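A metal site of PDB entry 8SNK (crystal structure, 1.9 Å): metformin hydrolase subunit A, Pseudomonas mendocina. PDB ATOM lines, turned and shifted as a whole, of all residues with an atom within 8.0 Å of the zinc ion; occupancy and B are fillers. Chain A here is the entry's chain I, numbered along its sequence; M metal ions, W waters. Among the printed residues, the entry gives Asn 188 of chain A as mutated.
The side-chain hydroxyl of Ser 280 is in hydrogen-bond range of the backbone carbonyl oxygen of Asp 277, 2.8 Å away. ND1 of His 159 lies within hydrogen-bond range of OD2 of Asp 184, at 3.0 Å. OD1 of Asn 289 sits at hydrogen-bond distance from N of Asp 279, at 3.2 Å. The side-chain carboxylate (OD1) of Asp 279 is in hydrogen-bond range of the backbone NH (N) of Cys 185. A ring nitrogen (NE2) of His 182 is in hydrogen-bond range of the side-chain carboxylate (OD2) of Asp 184 (2.9 Å). N of Asp 277 lies within hydrogen-bond range of O of Val 183 (2.8 Å). A ring nitrogen (ND1) of His 159 sits close to the side-chain carboxylate (OD2) of Asp 277. OD2 of Asp 184 lies within hydrogen-bond range of ND2 of Asn 188.
Within 4 Å of the zinc ion: Asp 184, His 186, Asp 277 and Asp 279. The nearest printed residue that does not touch the zinc ion is His 159 (4.5 Å).
The side-chain carboxylate (OD2) of Asp 277 is bound to the zinc ion, 2.1 Å away. OD1 of Asp 184 is bound to the zinc ion. The zinc ion is bound by water W1. The side-chain carboxylate (OD2) of Asp 279 is bound to the zinc ion, 2.2 Å away. ND1 of His 186 is bound to the zinc ion, 2.4 Å away. Slightly farther from the zinc ion lies OD1 of Asp 279 (2.7 Å).
Water W1 bridges ND2 of Asn 188 (3.1 Å) and OD2 of Asp 184 (3.5 Å).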
ATOM      1  N   VAL A  83     -35.295  33.812  -0.975  1.00  0.00           N
ATOM      2  CA  VAL A  83     -35.112  32.814   0.101  1.00  0.00           C
ATOM      3  C   VAL A  83     -35.115  33.487   1.495  1.00  0.00           C
ATOM      4  O   VAL A  83     -36.167  33.564   2.132  1.00  0.00           O
ATOM      5  CB  VAL A  83     -33.933  31.845  -0.154  1.00  0.00           C
ATOM      6  CG1 VAL A  83     -34.326  30.732  -1.109  1.00  0.00           C
ATOM      7  CG2 VAL A  83     -32.652  32.490  -0.673  1.00  0.00           C
ATOM      8  N   HIS A 159     -27.746  36.172  -4.754  1.00  0.00           N
ATOM      9  CA  HIS A 159     -27.398  35.673  -6.079  1.00  0.00           C
ATOM     10  C   HIS A 159     -28.068  36.466  -7.212  1.00  0.00           C
ATOM     11  O   HIS A 159     -27.993  36.021  -8.371  1.00  0.00           O
ATOM     12  CB  HIS A 159     -27.690  34.181  -6.249  1.00  0.00           C
ATOM     13  CG  HIS A 159     -26.609  33.620  -7.122  1.00  0.00           C
ATOM     14  ND1 HIS A 159     -26.299  32.265  -7.155  1.00  0.00           N
ATOM     15  CD2 HIS A 159     -25.662  34.223  -7.887  1.00  0.00           C
ATOM     16  CE1 HIS A 159     -25.251  32.071  -7.947  1.00  0.00           C
ATOM     17  NE2 HIS A 159     -24.835  33.239  -8.405  1.00  0.00           N
ATOM     18  N   HIS A 182     -21.532  29.466 -14.124  1.00  0.00           N
ATOM     19  CA  HIS A 182     -22.384  29.550 -12.961  1.00  0.00           C
ATOM     20  C   HIS A 182     -22.225  28.257 -12.178  1.00  0.00           C
ATOM     21  O   HIS A 182     -22.619  27.198 -12.639  1.00  0.00           O
ATOM     22  CB  HIS A 182     -23.802  29.908 -13.412  1.00  0.00           C
ATOM     23  CG  HIS A 182     -24.793  30.149 -12.343  1.00  0.00           C
ATOM     24  ND1 HIS A 182     -25.579  31.281 -12.387  1.00  0.00           N
ATOM     25  CD2 HIS A 182     -25.171  29.465 -11.257  1.00  0.00           C
ATOM     26  CE1 HIS A 182     -26.373  31.280 -11.321  1.00  0.00           C
ATOM     27  NE2 HIS A 182     -26.169  30.181 -10.638  1.00  0.00           N
ATOM     28  N   VAL A 183     -21.730  28.360 -10.932  1.00  0.00           N
ATOM     29  CA  VAL A 183     -21.527  27.211 -10.062  1.00  0.00           C
ATOM     30  C   VAL A 183     -22.357  27.372  -8.790  1.00  0.00           C
ATOM     31  O   VAL A 183     -22.223  28.355  -8.049  1.00  0.00           O
ATOM     32  CB  VAL A 183     -20.042  27.046  -9.751  1.00  0.00           C
ATOM     33  CG1 VAL A 183     -19.742  25.906  -8.758  1.00  0.00           C
ATOM     34  CG2 VAL A 183     -19.226  26.918 -11.031  1.00  0.00           C
ATOM     35  N   ASP A 184     -23.283  26.435  -8.606  1.00  0.00           N
ATOM     36  CA  ASP A 184     -24.412  26.630  -7.723  1.00  0.00           C
ATOM     37  C   ASP A 184     -25.003  25.242  -7.471  1.00  0.00           C
ATOM     38  O   ASP A 184     -25.054  24.442  -8.397  1.00  0.00           O
ATOM     39  CB  ASP A 184     -25.350  27.654  -8.369  1.00  0.00           C
ATOM     40  CG  ASP A 184     -26.345  28.355  -7.477  1.00  0.00           C
ATOM     41  OD1 ASP A 184     -26.676  27.824  -6.352  1.00  0.00           O
ATOM     42  OD2 ASP A 184     -26.831  29.438  -7.942  1.00  0.00           O
ATOM     43  N   CYS A 185     -25.511  24.993  -6.254  1.00  0.00           N
ATOM     44  CA  CYS A 185     -26.446  23.915  -6.002  1.00  0.00           C
ATOM     45  C   CYS A 185     -27.683  24.089  -6.875  1.00  0.00           C
ATOM     46  O   CYS A 185     -28.323  23.108  -7.233  1.00  0.00           O
ATOM     47  CB  CYS A 185     -26.934  23.944  -4.564  1.00  0.00           C
ATOM     48  SG  CYS A 185     -27.805  22.424  -4.172  1.00  0.00           S
ATOM     49  N   HIS A 186     -28.064  25.359  -7.088  1.00  0.00           N
ATOM     50  CA  HIS A 186     -29.321  25.716  -7.745  1.00  0.00           C
ATOM     51  C   HIS A 186     -29.096  26.170  -9.186  1.00  0.00           C
ATOM     52  O   HIS A 186     -28.164  26.927  -9.437  1.00  0.00           O
ATOM     53  CB  HIS A 186     -29.993  26.874  -7.008  1.00  0.00           C
ATOM     54  CG  HIS A 186     -30.109  26.541  -5.558  1.00  0.00           C
ATOM     55  ND1 HIS A 186     -29.503  27.238  -4.543  1.00  0.00           N
ATOM     56  CD2 HIS A 186     -30.742  25.508  -4.961  1.00  0.00           C
ATOM     57  CE1 HIS A 186     -29.792  26.660  -3.381  1.00  0.00           C
ATOM     58  NE2 HIS A 186     -30.527  25.587  -3.618  1.00  0.00           N
ATOM     59  N   LEU A 187     -29.998  25.723 -10.093  1.00  0.00           N
ATOM     60  CA  LEU A 187     -29.873  25.963 -11.532  1.00  0.00           C
ATOM     61  C   LEU A 187     -30.125  27.444 -11.900  1.00  0.00           C
ATOM     62  O   LEU A 187     -29.599  27.932 -12.902  1.00  0.00           O
ATOM     63  CB  LEU A 187     -30.837  24.997 -12.274  1.00  0.00           C
ATOM     64  CG  LEU A 187     -30.427  23.522 -12.282  1.00  0.00           C
ATOM     65  CD1 LEU A 187     -31.495  22.645 -12.903  1.00  0.00           C
ATOM     66  CD2 LEU A 187     -29.106  23.312 -13.019  1.00  0.00           C
ATOM     67  N   ASN A 188     -30.906  28.177 -11.076  1.00  0.00           N
ATOM     68  CA  ASN A 188     -31.102  29.617 -11.179  1.00  0.00           C
ATOM     69  C   ASN A 188     -31.403  30.067 -12.609  1.00  0.00           C
ATOM     70  O   ASN A 188     -30.726  30.949 -13.140  1.00  0.00           O
ATOM     71  CB  ASN A 188     -29.913  30.389 -10.577  1.00  0.00           C
ATOM     72  CG  ASN A 188     -30.061  30.480  -9.081  1.00  0.00           C
ATOM     73  OD1 ASN A 188     -31.049  29.973  -8.540  1.00  0.00           O
ATOM     74  ND2 ASN A 188     -29.122  31.153  -8.407  1.00  0.00           N
ATOM     75  N   ASN A 200     -32.695  36.758  -7.711  1.00  0.00           N
ATOM     76  CA  ASN A 200     -31.570  35.825  -7.560  1.00  0.00           C
ATOM     77  C   ASN A 200     -31.766  34.492  -8.303  1.00  0.00           C
ATOM     78  O   ASN A 200     -30.778  33.748  -8.439  1.00  0.00           O
ATOM     79  CB  ASN A 200     -31.324  35.555  -6.070  1.00  0.00           C
ATOM     80  CG  ASN A 200     -32.411  34.642  -5.510  1.00  0.00           C
ATOM     81  OD1 ASN A 200     -33.575  35.029  -5.382  1.00  0.00           O
ATOM     82  ND2 ASN A 200     -32.069  33.399  -5.228  1.00  0.00           N
ATOM     83  N   HIS A 220     -23.160  25.573 -16.467  1.00  0.00           N
ATOM     84  CA  HIS A 220     -23.535  25.469 -15.080  1.00  0.00           C
ATOM     85  C   HIS A 220     -22.853  24.239 -14.485  1.00  0.00           C
ATOM     86  O   HIS A 220     -22.881  23.191 -15.123  1.00  0.00           O
ATOM     87  CB  HIS A 220     -25.035  25.305 -14.947  1.00  0.00           C
ATOM     88  CG  HIS A 220     -25.529  25.535 -13.539  1.00  0.00           C
ATOM     89  ND1 HIS A 220     -25.399  24.573 -12.573  1.00  0.00           N
ATOM     90  CD2 HIS A 220     -26.199  26.568 -12.989  1.00  0.00           C
ATOM     91  CE1 HIS A 220     -25.946  25.027 -11.458  1.00  0.00           C
ATOM     92  NE2 HIS A 220     -26.440  26.240 -11.670  1.00  0.00           N
ATOM     93  N   LEU A 227     -34.400  21.794  -4.823  1.00  0.00           N
ATOM     94  CA  LEU A 227     -34.722  23.208  -4.887  1.00  0.00           C
ATOM     95  C   LEU A 227     -34.349  23.678  -6.292  1.00  0.00           C
ATOM     96  O   LEU A 227     -33.380  24.415  -6.468  1.00  0.00           O
ATOM     97  CB  LEU A 227     -34.013  23.995  -3.783  1.00  0.00           C
ATOM     98  CG  LEU A 227     -34.696  25.294  -3.320  1.00  0.00           C
ATOM     99  CD1 LEU A 227     -33.851  26.015  -2.267  1.00  0.00           C
ATOM    100  CD2 LEU A 227     -34.994  26.237  -4.484  1.00  0.00           C
ATOM    101  N   ASN A 228     -35.114  23.207  -7.266  1.00  0.00           N
ATOM    102  CA  ASN A 228     -34.799  23.315  -8.691  1.00  0.00           C
ATOM    103  C   ASN A 228     -36.057  23.034  -9.516  1.00  0.00           C
ATOM    104  O   ASN A 228     -36.248  21.920 -10.021  1.00  0.00           O
ATOM    105  CB  ASN A 228     -33.656  22.354  -9.061  1.00  0.00           C
ATOM    106  CG  ASN A 228     -32.267  22.889  -8.744  1.00  0.00           C
ATOM    107  OD1 ASN A 228     -31.885  23.928  -9.298  1.00  0.00           O
ATOM    108  ND2 ASN A 228     -31.473  22.141  -7.979  1.00  0.00           N
ATOM    109  N   TRP A 232     -36.286  25.543 -14.600  1.00  0.00           N
ATOM    110  CA  TRP A 232     -34.868  25.888 -14.476  1.00  0.00           C
ATOM    111  C   TRP A 232     -34.008  24.882 -15.264  1.00  0.00           C
ATOM    112  O   TRP A 232     -32.998  25.248 -15.835  1.00  0.00           O
ATOM    113  CB  TRP A 232     -34.380  25.984 -13.024  1.00  0.00           C
ATOM    114  CG  TRP A 232     -35.076  27.012 -12.174  1.00  0.00           C
ATOM    115  CD1 TRP A 232     -36.132  27.810 -12.495  1.00  0.00           C
ATOM    116  CD2 TRP A 232     -34.730  27.332 -10.820  1.00  0.00           C
ATOM    117  NE1 TRP A 232     -36.495  28.566 -11.410  1.00  0.00           N
ATOM    118  CE2 TRP A 232     -35.631  28.319 -10.380  1.00  0.00           C
ATOM    119  CE3 TRP A 232     -33.782  26.847  -9.915  1.00  0.00           C
ATOM    120  CZ2 TRP A 232     -35.572  28.862  -9.089  1.00  0.00           C
ATOM    121  CZ3 TRP A 232     -33.728  27.382  -8.642  1.00  0.00           C
ATOM    122  CH2 TRP A 232     -34.620  28.369  -8.238  1.00  0.00           C
ATOM    123  N   TRP A 276     -20.032  32.291  -8.447  1.00  0.00           N
ATOM    124  CA  TRP A 276     -19.842  31.092  -7.609  1.00  0.00           C
ATOM    125  C   TRP A 276     -20.678  31.262  -6.350  1.00  0.00           C
ATOM    126  O   TRP A 276     -20.327  32.055  -5.459  1.00  0.00           O
ATOM    127  CB  TRP A 276     -18.364  30.932  -7.276  1.00  0.00           C
ATOM    128  CG  TRP A 276     -17.953  29.596  -6.734  1.00  0.00           C
ATOM    129  CD1 TRP A 276     -18.756  28.546  -6.400  1.00  0.00           C
ATOM    130  CD2 TRP A 276     -16.605  29.172  -6.537  1.00  0.00           C
ATOM    131  NE1 TRP A 276     -17.996  27.490  -5.965  1.00  0.00           N
ATOM    132  CE2 TRP A 276     -16.672  27.838  -6.057  1.00  0.00           C
ATOM    133  CE3 TRP A 276     -15.357  29.780  -6.684  1.00  0.00           C
ATOM    134  CZ2 TRP A 276     -15.525  27.134  -5.723  1.00  0.00           C
ATOM    135  CZ3 TRP A 276     -14.211  29.061  -6.399  1.00  0.00           C
ATOM    136  CH2 TRP A 276     -14.311  27.765  -5.891  1.00  0.00           C
ATOM    137  N   ASP A 277     -21.764  30.487  -6.257  1.00  0.00           N
ATOM    138  CA  ASP A 277     -22.570  30.439  -5.035  1.00  0.00           C
ATOM    139  C   ASP A 277     -21.897  29.567  -3.961  1.00  0.00           C
ATOM    140  O   ASP A 277     -21.484  28.446  -4.251  1.00  0.00           O
ATOM    141  CB  ASP A 277     -23.922  29.835  -5.359  1.00  0.00           C
ATOM    142  CG  ASP A 277     -24.992  30.142  -4.358  1.00  0.00           C
ATOM    143  OD1 ASP A 277     -24.685  30.184  -3.109  1.00  0.00           O
ATOM    144  OD2 ASP A 277     -26.158  30.248  -4.792  1.00  0.00           O
ATOM    145  N   THR A 278     -21.861  30.045  -2.738  1.00  0.00           N
ATOM    146  CA  THR A 278     -21.282  29.298  -1.627  1.00  0.00           C
ATOM    147  C   THR A 278     -22.135  28.070  -1.287  1.00  0.00           C
ATOM    148  O   THR A 278     -21.611  27.152  -0.640  1.00  0.00           O
ATOM    149  CB  THR A 278     -21.015  30.176  -0.396  1.00  0.00           C
ATOM    150  OG1 THR A 278     -22.236  30.814  -0.023  1.00  0.00           O
ATOM    151  CG2 THR A 278     -19.934  31.200  -0.663  1.00  0.00           C
ATOM    152  N   ASP A 279     -23.397  27.988  -1.763  1.00  0.00           N
ATOM    153  CA  ASP A 279     -24.147  26.759  -1.534  1.00  0.00           C
ATOM    154  C   ASP A 279     -23.801  25.622  -2.489  1.00  0.00           C
ATOM    155  O   ASP A 279     -24.355  24.519  -2.325  1.00  0.00           O
ATOM    156  CB  ASP A 279     -25.631  27.027  -1.515  1.00  0.00           C
ATOM    157  CG  ASP A 279     -26.235  27.453  -2.807  1.00  0.00           C
ATOM    158  OD1 ASP A 279     -25.688  27.152  -3.847  1.00  0.00           O
ATOM    159  OD2 ASP A 279     -27.236  28.162  -2.698  1.00  0.00           O
ATOM    160  N   SER A 280     -22.856  25.850  -3.433  1.00  0.00           N
ATOM    161  CA  SER A 280     -22.225  24.774  -4.189  1.00  0.00           C
ATOM    162  C   SER A 280     -21.379  23.880  -3.273  1.00  0.00           C
ATOM    163  O   SER A 280     -21.177  22.699  -3.517  1.00  0.00           O
ATOM    164  CB  SER A 280     -21.414  25.314  -5.345  1.00  0.00           C
ATOM    165  OG  SER A 280     -20.238  25.992  -4.937  1.00  0.00           O
ATOM    166  N   ASN A 289     -25.234  29.849   5.147  1.00  0.00           N
ATOM    167  CA  ASN A 289     -25.633  30.137   3.787  1.00  0.00           C
ATOM    168  C   ASN A 289     -27.145  30.315   3.760  1.00  0.00           C
ATOM    169  O   ASN A 289     -27.809  29.810   4.666  1.00  0.00           O
ATOM    170  CB  ASN A 289     -25.079  29.051   2.859  1.00  0.00           C
ATOM    171  CG  ASN A 289     -25.372  29.305   1.401  1.00  0.00           C
ATOM    172  OD1 ASN A 289     -24.491  29.724   0.661  1.00  0.00           O
ATOM    173  ND2 ASN A 289     -26.603  29.053   0.992  1.00  0.00           N
ATOM    174  N   SER A 290     -27.657  31.080   2.777  1.00  0.00           N
ATOM    175  CA  SER A 290     -29.081  31.387   2.705  1.00  0.00           C
ATOM    176  C   SER A 290     -29.910  30.106   2.511  1.00  0.00           C
ATOM    177  O   SER A 290     -31.010  29.983   3.027  1.00  0.00           O
ATOM    178  CB  SER A 290     -29.420  32.358   1.566  1.00  0.00           C
ATOM    179  OG  SER A 290     -28.295  33.123   1.163  1.00  0.00           O
ATOM    180  N   ALA A 291     -29.427  29.194   1.660  1.00  0.00           N
ATOM    181  CA  ALA A 291     -30.088  27.912   1.424  1.00  0.00           C
ATOM    182  C   ALA A 291     -29.048  26.804   1.322  1.00  0.00           C
ATOM    183  O   ALA A 291     -28.705  26.389   0.224  1.00  0.00           O
ATOM    184  CB  ALA A 291     -30.911  27.951   0.183  1.00  0.00           C
ATOM    185  N   PRO A 292     -28.523  26.275   2.444  1.00  0.00           N
ATOM    186  CA  PRO A 292     -27.381  25.364   2.380  1.00  0.00           C
ATOM    187  C   PRO A 292     -27.829  23.960   1.979  1.00  0.00           C
ATOM    188  O   PRO A 292     -28.968  23.625   2.210  1.00  0.00           O
ATOM    189  CB  PRO A 292     -26.835  25.386   3.819  1.00  0.00           C
ATOM    190  CG  PRO A 292     -28.053  25.786   4.697  1.00  0.00           C
ATOM    191  CD  PRO A 292     -29.052  26.459   3.802  1.00  0.00           C
ATOM    192  N   GLU A 293     -26.907  23.112   1.479  1.00  0.00           N
ATOM    193  CA  GLU A 293     -27.295  21.863   0.843  1.00  0.00           C
ATOM    194  C   GLU A 293     -26.215  20.809   1.054  1.00  0.00           C
ATOM    195  O   GLU A 293     -25.060  21.116   0.795  1.00  0.00           O
ATOM    196  CB  GLU A 293     -27.423  22.111  -0.665  1.00  0.00           C
ATOM    197  CG  GLU A 293     -28.593  22.979  -1.066  1.00  0.00           C
ATOM    198  CD  GLU A 293     -29.918  22.234  -1.054  1.00  0.00           C
ATOM    199  OE1 GLU A 293     -29.913  20.997  -0.758  1.00  0.00           O
ATOM    200  OE2 GLU A 293     -30.949  22.906  -1.312  1.00  0.00           O
ATOM    201  N   VAL A 320     -21.145  34.495  -3.752  1.00  0.00           N
ATOM    202  CA  VAL A 320     -22.381  34.996  -3.198  1.00  0.00           C
ATOM    203  C   VAL A 320     -22.947  34.078  -2.107  1.00  0.00           C
ATOM    204  O   VAL A 320     -22.555  32.937  -2.003  1.00  0.00           O
ATOM    205  CB  VAL A 320     -23.435  35.185  -4.313  1.00  0.00           C
ATOM    206  CG1 VAL A 320     -22.964  36.175  -5.368  1.00  0.00           C
ATOM    207  CG2 VAL A 320     -23.835  33.885  -4.959  1.00  0.00           C
ATOM    208  N   GLU A 321     -23.920  34.645  -1.349  1.00  0.00           N
ATOM    209  CA  GLU A 321     -24.877  33.968  -0.496  1.00  0.00           C
ATOM    210  C   GLU A 321     -24.285  33.522   0.841  1.00  0.00           C
ATOM    211  O   GLU A 321     -24.940  32.831   1.604  1.00  0.00           O
ATOM    212  CB  GLU A 321     -25.546  32.774  -1.155  1.00  0.00           C
ATOM    213  CG  GLU A 321     -26.564  33.118  -2.240  1.00  0.00           C
ATOM    214  CD  GLU A 321     -27.761  33.984  -1.884  1.00  0.00           C
ATOM    215  OE1 GLU A 321     -27.889  34.440  -0.701  1.00  0.00           O
ATOM    216  OE2 GLU A 321     -28.567  34.273  -2.825  1.00  0.00           O
HETATM  217 ZN    ZN M   1     -27.685  28.772  -4.725  1.00  0.00          ZN
HETATM  218  O   HOH W   1     -28.934  30.416  -5.356  1.00  0.00           O
